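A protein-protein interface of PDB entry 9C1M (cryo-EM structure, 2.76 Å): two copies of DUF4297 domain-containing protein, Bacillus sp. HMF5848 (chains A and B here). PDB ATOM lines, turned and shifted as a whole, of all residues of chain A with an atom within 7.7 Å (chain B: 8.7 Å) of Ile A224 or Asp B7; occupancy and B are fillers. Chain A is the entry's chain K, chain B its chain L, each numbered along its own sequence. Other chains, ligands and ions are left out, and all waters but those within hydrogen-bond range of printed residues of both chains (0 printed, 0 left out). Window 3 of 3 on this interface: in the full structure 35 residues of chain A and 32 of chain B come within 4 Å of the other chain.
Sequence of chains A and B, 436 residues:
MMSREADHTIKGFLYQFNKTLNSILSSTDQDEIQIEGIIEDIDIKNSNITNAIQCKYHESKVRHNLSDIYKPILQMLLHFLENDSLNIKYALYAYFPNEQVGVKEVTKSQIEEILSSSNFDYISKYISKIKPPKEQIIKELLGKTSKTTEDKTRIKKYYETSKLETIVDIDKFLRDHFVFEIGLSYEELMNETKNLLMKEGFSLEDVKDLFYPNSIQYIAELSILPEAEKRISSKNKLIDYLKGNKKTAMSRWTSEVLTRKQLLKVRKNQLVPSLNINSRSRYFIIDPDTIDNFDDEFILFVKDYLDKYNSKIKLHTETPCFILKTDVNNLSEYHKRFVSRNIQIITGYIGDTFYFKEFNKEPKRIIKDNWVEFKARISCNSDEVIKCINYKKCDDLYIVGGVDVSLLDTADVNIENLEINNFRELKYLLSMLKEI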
ATOM      1  N   PHE A  13      19.399 -17.475  10.094  1.00  0.00           N
ATOM      2  CA  PHE A  13      20.230 -17.928  11.206  1.00  0.00           C
ATOM      3  C   PHE A  13      19.542 -19.037  11.995  1.00  0.00           C
ATOM      4  O   PHE A  13      20.193 -19.997  12.425  1.00  0.00           O
ATOM      5  CB  PHE A  13      20.580 -16.751  12.114  1.00  0.00           C
ATOM      6  CG  PHE A  13      21.773 -15.966  11.650  1.00  0.00           C
ATOM      7  CD1 PHE A  13      22.964 -16.607  11.350  1.00  0.00           C
ATOM      8  CD2 PHE A  13      21.704 -14.591  11.510  1.00  0.00           C
ATOM      9  CE1 PHE A  13      24.064 -15.890  10.918  1.00  0.00           C
ATOM     10  CE2 PHE A  13      22.802 -13.869  11.081  1.00  0.00           C
ATOM     11  CZ  PHE A  13      23.983 -14.519  10.785  1.00  0.00           C
ATOM     12  N   GLN A  16      19.956 -22.142  10.013  1.00  0.00           N
ATOM     13  CA  GLN A  16      21.298 -22.687  10.198  1.00  0.00           C
ATOM     14  C   GLN A  16      21.419 -23.412  11.535  1.00  0.00           C
ATOM     15  O   GLN A  16      22.028 -24.488  11.617  1.00  0.00           O
ATOM     16  CB  GLN A  16      22.335 -21.569  10.098  1.00  0.00           C
ATOM     17  CG  GLN A  16      23.755 -22.000  10.429  1.00  0.00           C
ATOM     18  CD  GLN A  16      24.729 -20.839  10.442  1.00  0.00           C
ATOM     19  OE1 GLN A  16      24.521 -19.832   9.766  1.00  0.00           O
ATOM     20  NE2 GLN A  16      25.800 -20.973  11.216  1.00  0.00           N
ATOM     21  N   PHE A  17      20.852 -22.830  12.596  1.00  0.00           N
ATOM     22  CA  PHE A  17      20.875 -23.483  13.902  1.00  0.00           C
ATOM     23  C   PHE A  17      20.121 -24.806  13.870  1.00  0.00           C
ATOM     24  O   PHE A  17      20.583 -25.809  14.427  1.00  0.00           O
ATOM     25  CB  PHE A  17      20.283 -22.556  14.964  1.00  0.00           C
ATOM     26  CG  PHE A  17      21.073 -21.298  15.184  1.00  0.00           C
ATOM     27  CD1 PHE A  17      22.422 -21.245  14.872  1.00  0.00           C
ATOM     28  CD2 PHE A  17      20.467 -20.168  15.705  1.00  0.00           C
ATOM     29  CE1 PHE A  17      23.150 -20.088  15.074  1.00  0.00           C
ATOM     30  CE2 PHE A  17      21.189 -19.008  15.909  1.00  0.00           C
ATOM     31  CZ  PHE A  17      22.532 -18.968  15.594  1.00  0.00           C
ATOM     32  N   ILE A  35      30.285 -26.211  15.887  1.00  0.00           N
ATOM     33  CA  ILE A  35      29.254 -25.236  15.550  1.00  0.00           C
ATOM     34  C   ILE A  35      29.927 -23.915  15.203  1.00  0.00           C
ATOM     35  O   ILE A  35      30.780 -23.426  15.953  1.00  0.00           O
ATOM     36  CB  ILE A  35      28.262 -25.071  16.710  1.00  0.00           C
ATOM     37  CG1 ILE A  35      27.797 -26.443  17.201  1.00  0.00           C
ATOM     38  CG2 ILE A  35      27.073 -24.228  16.280  1.00  0.00           C
ATOM     39  CD1 ILE A  35      27.201 -26.425  18.583  1.00  0.00           C
ATOM     40  N   GLU A  36      29.543 -23.338  14.066  1.00  0.00           N
ATOM     41  CA  GLU A  36      30.218 -22.171  13.498  1.00  0.00           C
ATOM     42  C   GLU A  36      31.710 -22.459  13.328  1.00  0.00           C
ATOM     43  O   GLU A  36      32.579 -21.775  13.871  1.00  0.00           O
ATOM     44  CB  GLU A  36      29.982 -20.922  14.353  1.00  0.00           C
ATOM     45  CG  GLU A  36      28.640 -20.253  14.110  1.00  0.00           C
ATOM     46  CD  GLU A  36      28.562 -19.578  12.755  1.00  0.00           C
ATOM     47  OE1 GLU A  36      29.619 -19.166  12.232  1.00  0.00           O
ATOM     48  OE2 GLU A  36      27.443 -19.461  12.210  1.00  0.00           O
ATOM     49  N   TYR A 218      21.501 -23.643  23.372  1.00  0.00           N
ATOM     50  CA  TYR A 218      22.858 -24.177  23.429  1.00  0.00           C
ATOM     51  C   TYR A 218      23.597 -23.949  22.115  1.00  0.00           C
ATOM     52  O   TYR A 218      24.772 -23.558  22.112  1.00  0.00           O
ATOM     53  CB  TYR A 218      22.799 -25.665  23.778  1.00  0.00           C
ATOM     54  CG  TYR A 218      24.135 -26.366  23.853  1.00  0.00           C
ATOM     55  CD1 TYR A 218      24.963 -26.207  24.957  1.00  0.00           C
ATOM     56  CD2 TYR A 218      24.556 -27.212  22.836  1.00  0.00           C
ATOM     57  CE1 TYR A 218      26.181 -26.855  25.035  1.00  0.00           C
ATOM     58  CE2 TYR A 218      25.770 -27.865  22.905  1.00  0.00           C
ATOM     59  CZ  TYR A 218      26.579 -27.684  24.009  1.00  0.00           C
ATOM     60  OH  TYR A 218      27.790 -28.331  24.081  1.00  0.00           O
ATOM     61  N   ILE A 219      22.917 -24.177  20.988  1.00  0.00           N
ATOM     62  CA  ILE A 219      23.522 -23.932  19.681  1.00  0.00           C
ATOM     63  C   ILE A 219      23.882 -22.460  19.528  1.00  0.00           C
ATOM     64  O   ILE A 219      24.977 -22.116  19.066  1.00  0.00           O
ATOM     65  CB  ILE A 219      22.578 -24.399  18.556  1.00  0.00           C
ATOM     66  CG1 ILE A 219      22.373 -25.915  18.608  1.00  0.00           C
ATOM     67  CG2 ILE A 219      23.116 -23.978  17.197  1.00  0.00           C
ATOM     68  CD1 ILE A 219      23.635 -26.715  18.420  1.00  0.00           C
ATOM     69  N   ALA A 220      22.965 -21.568  19.915  1.00  0.00           N
ATOM     70  CA  ALA A 220      23.225 -20.137  19.792  1.00  0.00           C
ATOM     71  C   ALA A 220      24.388 -19.705  20.678  1.00  0.00           C
ATOM     72  O   ALA A 220      25.221 -18.888  20.269  1.00  0.00           O
ATOM     73  CB  ALA A 220      21.964 -19.344  20.134  1.00  0.00           C
ATOM     74  N   GLU A 221      24.456 -20.240  21.900  1.00  0.00           N
ATOM     75  CA  GLU A 221      25.541 -19.886  22.809  1.00  0.00           C
ATOM     76  C   GLU A 221      26.884 -20.388  22.293  1.00  0.00           C
ATOM     77  O   GLU A 221      27.896 -19.688  22.405  1.00  0.00           O
ATOM     78  CB  GLU A 221      25.259 -20.439  24.205  1.00  0.00           C
ATOM     79  CG  GLU A 221      24.203 -19.662  24.975  1.00  0.00           C
ATOM     80  CD  GLU A 221      23.896 -20.276  26.326  1.00  0.00           C
ATOM     81  OE1 GLU A 221      24.543 -21.283  26.685  1.00  0.00           O
ATOM     82  OE2 GLU A 221      23.007 -19.753  27.031  1.00  0.00           O
ATOM     83  N   LEU A 222      26.918 -21.599  21.729  1.00  0.00           N
ATOM     84  CA  LEU A 222      28.172 -22.108  21.186  1.00  0.00           C
ATOM     85  C   LEU A 222      28.549 -21.440  19.871  1.00  0.00           C
ATOM     86  O   LEU A 222      29.724 -21.466  19.492  1.00  0.00           O
ATOM     87  CB  LEU A 222      28.098 -23.623  20.990  1.00  0.00           C
ATOM     88  CG  LEU A 222      28.118 -24.493  22.250  1.00  0.00           C
ATOM     89  CD1 LEU A 222      28.548 -25.906  21.899  1.00  0.00           C
ATOM     90  CD2 LEU A 222      29.021 -23.904  23.319  1.00  0.00           C
ATOM     91  N   SER A 223      27.584 -20.843  19.167  1.00  0.00           N
ATOM     92  CA  SER A 223      27.880 -20.205  17.890  1.00  0.00           C
ATOM     93  C   SER A 223      28.650 -18.901  18.050  1.00  0.00           C
ATOM     94  O   SER A 223      29.345 -18.489  17.114  1.00  0.00           O
ATOM     95  CB  SER A 223      26.583 -19.947  17.120  1.00  0.00           C
ATOM     96  OG  SER A 223      25.924 -21.163  16.809  1.00  0.00           O
ATOM     97  N   ILE A 224      28.547 -18.244  19.208  1.00  0.00           N
ATOM     98  CA  ILE A 224      29.155 -16.929  19.403  1.00  0.00           C
ATOM     99  C   ILE A 224      30.533 -16.995  20.046  1.00  0.00           C
ATOM    100  O   ILE A 224      31.201 -15.953  20.149  1.00  0.00           O
ATOM    101  CB  ILE A 224      28.249 -16.018  20.256  1.00  0.00           C
ATOM    102  CG1 ILE A 224      28.192 -16.535  21.694  1.00  0.00           C
ATOM    103  CG2 ILE A 224      26.855 -15.950  19.664  1.00  0.00           C
ATOM    104  CD1 ILE A 224      27.613 -15.552  22.675  1.00  0.00           C
ATOM    105  N   LEU A 225      30.977 -18.165  20.481  1.00  0.00           N
ATOM    106  CA  LEU A 225      32.232 -18.262  21.220  1.00  0.00           C
ATOM    107  C   LEU A 225      33.412 -17.964  20.305  1.00  0.00           C
ATOM    108  O   LEU A 225      33.552 -18.606  19.257  1.00  0.00           O
ATOM    109  CB  LEU A 225      32.372 -19.649  21.837  1.00  0.00           C
ATOM    110  CG  LEU A 225      31.358 -19.972  22.936  1.00  0.00           C
ATOM    111  CD1 LEU A 225      31.590 -21.365  23.491  1.00  0.00           C
ATOM    112  CD2 LEU A 225      31.417 -18.933  24.045  1.00  0.00           C
ATOM    113  N   PRO A 226      34.272 -16.999  20.647  1.00  0.00           N
ATOM    114  CA  PRO A 226      35.427 -16.708  19.781  1.00  0.00           C
ATOM    115  C   PRO A 226      36.390 -17.874  19.638  1.00  0.00           C
ATOM    116  O   PRO A 226      36.996 -18.036  18.572  1.00  0.00           O
ATOM    117  CB  PRO A 226      36.088 -15.509  20.476  1.00  0.00           C
ATOM    118  CG  PRO A 226      35.645 -15.601  21.900  1.00  0.00           C
ATOM    119  CD  PRO A 226      34.256 -16.162  21.858  1.00  0.00           C
ATOM    120  N   GLU A 227      36.550 -18.691  20.677  1.00  0.00           N
ATOM    121  CA  GLU A 227      37.480 -19.810  20.624  1.00  0.00           C
ATOM    122  C   GLU A 227      36.898 -20.939  19.781  1.00  0.00           C
ATOM    123  O   GLU A 227      35.747 -21.341  19.975  1.00  0.00           O
ATOM    124  CB  GLU A 227      37.797 -20.309  22.033  1.00  0.00           C
ATOM    125  CG  GLU A 227      38.465 -19.272  22.921  1.00  0.00           C
ATOM    126  CD  GLU A 227      38.550 -19.715  24.368  1.00  0.00           C
ATOM    127  OE1 GLU A 227      38.778 -20.919  24.609  1.00  0.00           O
ATOM    128  OE2 GLU A 227      38.388 -18.860  25.264  1.00  0.00           O
ATOM    129  N   ARG A 231      33.788 -24.224  20.579  1.00  0.00           N
ATOM    130  CA  ARG A 231      32.652 -24.408  19.687  1.00  0.00           C
ATOM    131  C   ARG A 231      32.466 -25.856  19.251  1.00  0.00           C
ATOM    132  O   ARG A 231      31.522 -26.147  18.510  1.00  0.00           O
ATOM    133  CB  ARG A 231      32.802 -23.512  18.453  1.00  0.00           C
ATOM    134  CG  ARG A 231      32.801 -22.027  18.771  1.00  0.00           C
ATOM    135  CD  ARG A 231      32.817 -21.184  17.506  1.00  0.00           C
ATOM    136  NE  ARG A 231      34.096 -21.261  16.812  1.00  0.00           N
ATOM    137  CZ  ARG A 231      34.478 -20.430  15.852  1.00  0.00           C
ATOM    138  NH1 ARG A 231      33.699 -19.442  15.443  1.00  0.00           N
ATOM    139  NH2 ARG A 231      35.671 -20.594  15.287  1.00  0.00           N
ATOM    140  N   ASP B   7      30.105 -15.222  13.543  1.00  0.00           N
ATOM    141  CA  ASP B   7      29.714 -15.342  14.943  1.00  0.00           C
ATOM    142  C   ASP B   7      29.306 -13.989  15.517  1.00  0.00           C
ATOM    143  O   ASP B   7      28.465 -13.913  16.413  1.00  0.00           O
ATOM    144  CB  ASP B   7      30.855 -15.942  15.767  1.00  0.00           C
ATOM    145  CG  ASP B   7      32.121 -15.110  15.707  1.00  0.00           C
ATOM    146  OD1 ASP B   7      32.358 -14.464  14.664  1.00  0.00           O
ATOM    147  OD2 ASP B   7      32.877 -15.102  16.700  1.00  0.00           O
ATOM    148  N   HIS B   8      29.914 -12.921  14.995  1.00  0.00           N
ATOM    149  CA  HIS B   8      29.600 -11.579  15.476  1.00  0.00           C
ATOM    150  C   HIS B   8      28.156 -11.200  15.168  1.00  0.00           C
ATOM    151  O   HIS B   8      27.478 -10.596  16.006  1.00  0.00           O
ATOM    152  CB  HIS B   8      30.567 -10.565  14.867  1.00  0.00           C
ATOM    153  CG  HIS B   8      31.951 -10.636  15.432  1.00  0.00           C
ATOM    154  ND1 HIS B   8      32.209 -10.558  16.784  1.00  0.00           N
ATOM    155  CD2 HIS B   8      33.155 -10.782  14.828  1.00  0.00           C
ATOM    156  CE1 HIS B   8      33.511 -10.650  16.989  1.00  0.00           C
ATOM    157  NE2 HIS B   8      34.107 -10.787  15.818  1.00  0.00           N
ATOM    158  N   THR B   9      27.671 -11.541  13.972  1.00  0.00           N
ATOM    159  CA  THR B   9      26.286 -11.242  13.625  1.00  0.00           C
ATOM    160  C   THR B   9      25.314 -12.021  14.506  1.00  0.00           C
ATOM    161  O   THR B   9      24.289 -11.481  14.939  1.00  0.00           O
ATOM    162  CB  THR B   9      26.035 -11.548  12.148  1.00  0.00           C
ATOM    163  OG1 THR B   9      27.098 -10.999  11.359  1.00  0.00           O
ATOM    164  CG2 THR B   9      24.718 -10.939  11.697  1.00  0.00           C
ATOM    165  N   ILE B  10      25.621 -13.292  14.778  1.00  0.00           N
ATOM    166  CA  ILE B  10      24.777 -14.092  15.662  1.00  0.00           C
ATOM    167  C   ILE B  10      24.767 -13.500  17.064  1.00  0.00           C
ATOM    168  O   ILE B  10      23.717 -13.423  17.716  1.00  0.00           O
ATOM    169  CB  ILE B  10      25.249 -15.558  15.667  1.00  0.00           C
ATOM    170  CG1 ILE B  10      24.928 -16.224  14.328  1.00  0.00           C
ATOM    171  CG2 ILE B  10      24.601 -16.328  16.806  1.00  0.00           C
ATOM    172  CD1 ILE B  10      25.582 -17.574  14.149  1.00  0.00           C
ATOM    173  N   LYS B  11      25.934 -13.076  17.554  1.00  0.00           N
ATOM    174  CA  LYS B  11      26.005 -12.459  18.874  1.00  0.00           C
ATOM    175  C   LYS B  11      25.204 -11.165  18.923  1.00  0.00           C
ATOM    176  O   LYS B  11      24.523 -10.886  19.914  1.00  0.00           O
ATOM    177  CB  LYS B  11      27.462 -12.207  19.260  1.00  0.00           C
ATOM    178  CG  LYS B  11      27.687 -12.055  20.756  1.00  0.00           C
ATOM    179  CD  LYS B  11      29.163 -12.131  21.106  1.00  0.00           C
ATOM    180  CE  LYS B  11      29.371 -12.156  22.612  1.00  0.00           C
ATOM    181  NZ  LYS B  11      30.805 -12.336  22.972  1.00  0.00           N
ATOM    182  N   GLY B  12      25.273 -10.361  17.860  1.00  0.00           N
ATOM    183  CA  GLY B  12      24.485  -9.139  17.816  1.00  0.00           C
ATOM    184  C   GLY B  12      22.991  -9.405  17.797  1.00  0.00           C
ATOM    185  O   GLY B  12      22.216  -8.711  18.459  1.00  0.00           O
ATOM    186  N   PHE B  13      22.565 -10.415  17.033  1.00  0.00           N
ATOM    187  CA  PHE B  13      21.149 -10.769  17.006  1.00  0.00           C
ATOM    188  C   PHE B  13      20.681 -11.279  18.363  1.00  0.00           C
ATOM    189  O   PHE B  13      19.573 -10.957  18.810  1.00  0.00           O
ATOM    190  CB  PHE B  13      20.889 -11.809  15.916  1.00  0.00           C
ATOM    191  CG  PHE B  13      20.630 -11.213  14.562  1.00  0.00           C
ATOM    192  CD1 PHE B  13      19.630 -10.272  14.386  1.00  0.00           C
ATOM    193  CD2 PHE B  13      21.387 -11.593  13.467  1.00  0.00           C
ATOM    194  CE1 PHE B  13      19.391  -9.718  13.142  1.00  0.00           C
ATOM    195  CE2 PHE B  13      21.152 -11.044  12.221  1.00  0.00           C
ATOM    196  CZ  PHE B  13      20.152 -10.107  12.059  1.00  0.00           C
ATOM    197  N   LEU B  14      21.514 -12.076  19.038  1.00  0.00           N
ATOM    198  CA  LEU B  14      21.171 -12.539  20.379  1.00  0.00           C
ATOM    199  C   LEU B  14      21.114 -11.379  21.366  1.00  0.00           C
ATOM    200  O   LEU B  14      20.267 -11.362  22.266  1.00  0.00           O
ATOM    201  CB  LEU B  14      22.174 -13.595  20.841  1.00  0.00           C
ATOM    202  CG  LEU B  14      22.058 -14.966  20.174  1.00  0.00           C
ATOM    203  CD1 LEU B  14      23.198 -15.873  20.609  1.00  0.00           C
ATOM    204  CD2 LEU B  14      20.711 -15.603  20.481  1.00  0.00           C
ATOM    205  N   TYR B  15      22.014 -10.404  21.216  1.00  0.00           N
ATOM    206  CA  TYR B  15      21.969  -9.207  22.049  1.00  0.00           C
ATOM    207  C   TYR B  15      20.676  -8.435  21.827  1.00  0.00           C
ATOM    208  O   TYR B  15      20.057  -7.952  22.783  1.00  0.00           O
ATOM    209  CB  TYR B  15      23.182  -8.325  21.746  1.00  0.00           C
ATOM    210  CG  TYR B  15      23.356  -7.148  22.679  1.00  0.00           C
ATOM    211  CD1 TYR B  15      23.972  -7.301  23.914  1.00  0.00           C
ATOM    212  CD2 TYR B  15      22.911  -5.881  22.323  1.00  0.00           C
ATOM    213  CE1 TYR B  15      24.139  -6.228  24.768  1.00  0.00           C
ATOM    214  CE2 TYR B  15      23.072  -4.802  23.170  1.00  0.00           C
ATOM    215  CZ  TYR B  15      23.685  -4.981  24.392  1.00  0.00           C
ATOM    216  OH  TYR B  15      23.847  -3.910  25.240  1.00  0.00           O
ATOM    217  N   ASN B  18      17.880 -10.364  23.538  1.00  0.00           N
ATOM    218  CA  ASN B  18      17.933 -10.177  24.984  1.00  0.00           C
ATOM    219  C   ASN B  18      17.458  -8.783  25.379  1.00  0.00           C
ATOM    220  O   ASN B  18      16.782  -8.621  26.400  1.00  0.00           O
ATOM    221  CB  ASN B  18      19.350 -10.432  25.495  1.00  0.00           C
ATOM    222  CG  ASN B  18      19.590 -11.888  25.841  1.00  0.00           C
ATOM    223  OD1 ASN B  18      19.197 -12.357  26.908  1.00  0.00           O
ATOM    224  ND2 ASN B  18      20.237 -12.613  24.936  1.00  0.00           N
ATOM    225  N   TYR B  57      25.508  -3.938  18.328  1.00  0.00           N
ATOM    226  CA  TYR B  57      26.519  -4.646  19.105  1.00  0.00           C
ATOM    227  C   TYR B  57      27.880  -4.394  18.472  1.00  0.00           C
ATOM    228  O   TYR B  57      28.080  -4.686  17.288  1.00  0.00           O
ATOM    229  CB  TYR B  57      26.211  -6.144  19.163  1.00  0.00           C
ATOM    230  CG  TYR B  57      26.913  -6.879  20.283  1.00  0.00           C
ATOM    231  CD1 TYR B  57      26.602  -6.621  21.611  1.00  0.00           C
ATOM    232  CD2 TYR B  57      27.880  -7.838  20.011  1.00  0.00           C
ATOM    233  CE1 TYR B  57      27.237  -7.292  22.638  1.00  0.00           C
ATOM    234  CE2 TYR B  57      28.520  -8.516  21.031  1.00  0.00           C
ATOM    235  CZ  TYR B  57      28.195  -8.239  22.343  1.00  0.00           C
ATOM    236  OH  TYR B  57      28.831  -8.910  23.362  1.00  0.00           O
ATOM    237  N   GLU B  59      31.150  -5.214  20.115  1.00  0.00           N
ATOM    238  CA  GLU B  59      32.132  -5.770  21.043  1.00  0.00           C
ATOM    239  C   GLU B  59      33.544  -5.726  20.470  1.00  0.00           C
ATOM    240  O   GLU B  59      34.517  -5.624  21.227  1.00  0.00           O
ATOM    241  CB  GLU B  59      31.753  -7.207  21.404  1.00  0.00           C
ATOM    242  CG  GLU B  59      32.614  -7.834  22.489  1.00  0.00           C
ATOM    243  CD  GLU B  59      32.202  -9.257  22.807  1.00  0.00           C
ATOM    244  OE1 GLU B  59      31.717  -9.955  21.892  1.00  0.00           O
ATOM    245  OE2 GLU B  59      32.365  -9.680  23.971  1.00  0.00           O
ATOM    246  N   SER B  60      33.679  -5.791  19.147  1.00  0.00           N
ATOM    247  CA  SER B  60      34.988  -5.828  18.508  1.00  0.00           C
ATOM    248  C   SER B  60      35.598  -4.446  18.307  1.00  0.00           C
ATOM    249  O   SER B  60      36.719  -4.354  17.796  1.00  0.00           O
ATOM    250  CB  SER B  60      34.893  -6.547  17.159  1.00  0.00           C
ATOM    251  OG  SER B  60      34.008  -5.871  16.283  1.00  0.00           O
ATOM    252  N   TYR B 186      26.696  -7.972  26.895  1.00  0.00           N
ATOM    253  CA  TYR B 186      25.773  -9.051  26.558  1.00  0.00           C
ATOM    254  C   TYR B 186      25.608 -10.019  27.725  1.00  0.00           C
ATOM    255  O   TYR B 186      24.491 -10.466  28.022  1.00  0.00           O
ATOM    256  CB  TYR B 186      26.274  -9.769  25.303  1.00  0.00           C
ATOM    257  CG  TYR B 186      25.495 -10.998  24.903  1.00  0.00           C
ATOM    258  CD1 TYR B 186      24.112 -10.962  24.781  1.00  0.00           C
ATOM    259  CD2 TYR B 186      26.146 -12.191  24.619  1.00  0.00           C
ATOM    260  CE1 TYR B 186      23.399 -12.083  24.403  1.00  0.00           C
ATOM    261  CE2 TYR B 186      25.441 -13.316  24.243  1.00  0.00           C
ATOM    262  CZ  TYR B 186      24.070 -13.258  24.135  1.00  0.00           C
ATOM    263  OH  TYR B 186      23.367 -14.379  23.760  1.00  0.00           O
ATOM    264  N   GLU B 187      26.709 -10.348  28.407  1.00  0.00           N
ATOM    265  CA  GLU B 187      26.617 -11.160  29.617  1.00  0.00           C
ATOM    266  C   GLU B 187      25.863 -10.420  30.717  1.00  0.00           C
ATOM    267  O   GLU B 187      25.014 -11.003  31.402  1.00  0.00           O
ATOM    268  CB  GLU B 187      28.014 -11.554  30.093  1.00  0.00           C
ATOM    269  CG  GLU B 187      28.734 -12.541  29.182  1.00  0.00           C
ATOM    270  CD  GLU B 187      29.365 -11.873  27.973  1.00  0.00           C
ATOM    271  OE1 GLU B 187      29.472 -10.629  27.968  1.00  0.00           O
ATOM    272  OE2 GLU B 187      29.752 -12.593  27.029  1.00  0.00           O
ATOM    273  N   MET B 190      22.150 -10.630  29.777  1.00  0.00           N
ATOM    274  CA  MET B 190      21.458 -11.850  30.183  1.00  0.00           C
ATOM    275  C   MET B 190      21.311 -11.920  31.698  1.00  0.00           C
ATOM    276  O   MET B 190      20.293 -12.417  32.195  1.00  0.00           O
ATOM    277  CB  MET B 190      22.172 -13.102  29.658  1.00  0.00           C
ATOM    278  CG  MET B 190      23.567 -13.343  30.207  1.00  0.00           C
ATOM    279  SD  MET B 190      24.394 -14.771  29.479  1.00  0.00           S
ATOM    280  CE  MET B 190      24.789 -14.148  27.848  1.00  0.00           C
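Ile A224 touches just these residues of chain B: Asp B7 (3.9 Å), Ile B10 (3.7 Å), Lys B11 (3.7 Å), Leu B14 (3.8 Å) and Tyr B186 (3.5 Å). Of the printed residues of chain A, Lys B11 touches Ile A224 (3.7 Å). Printed residues of chain B within 4 Å of Ala A220: Leu B14 (3.6 Å). Printed residues of chain B within 4 Å of Glu A36: Ile B10 (3.3 Å). Ile A35 touches none of the printed residues of chain B. Leu A225 touches none of the printed residues of chain B. The nearest residue of chain B that does not touch Ile A224 is Glu B187 (5.7 Å). The nearest printed residue of chain B that does not touch Phe A13 is Asp B7 (6.6 Å).
Phe A13 touches its own counterpart, Phe B13. 1 position is printed for both chains.
Printed residues of chain B that touch a printed residue of chain A: Asp B7, Thr B9, Ile B10, Lys B11, Phe B13, Leu B14 and Tyr B186. Hydrophobic or aromatic side chains of chain B that line the printed part of chain A: Ile B10, Phe B13, Leu B14 and Tyr B186. Among the printed residues, 13 pairs touch across the chains. Among the printed residues, no Asp or Glu carboxylate lies within 4 Å of a Lys or Arg side-chain nitrogen of the other chain.
The side-chain amide nitrogen of Gln A16 sits at hydrogen-bond distance from the side-chain carboxylate of Glu A36. The backbone carbonyl oxygen (O) of Glu A36 is in hydrogen-bond range of the guanidinium group (NH1) of Arg A231, 3.0 Å away. The backbone carbonyl oxygen of Ile A219 sits at hydrogen-bond distance from the side-chain hydroxyl of Ser A223. The side-chain carboxylate (OE1) of Glu B59 is in salt-bridge range of the side-chain amino group (NZ) of Lys B11, 2.8 Å away. The side-chain amide nitrogen (ND2) of Asn B18 lies within hydrogen-bond range of the backbone carbonyl oxygen (O) of Leu B14, 2.9 Å away.
Among the printed residues, pairs that only touch across the chains: Ser A223 with Asp B7 (3.3 Å), Glu A36 with Ile B10 (3.3 Å), Phe A13 with Phe B13 (3.5 Å), Ile A224 with Tyr B186 (3.5 Å), Phe A13 with Ile B10 (3.5 Å), Phe A13 with Thr B9 (3.6 Å), Phe A17 with Ile B10 (3.6 Å), Ala A220 with Leu B14 (3.6 Å), Ile A224 with Ile B10 (3.7 Å), Ile A224 with Lys B11 (3.7 Å), Ile A224 with Leu B14 (3.8 Å), Ile A224 with Asp B7 (3.9 Å) and Ser A223 with Ile B10 (3.9 Å).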
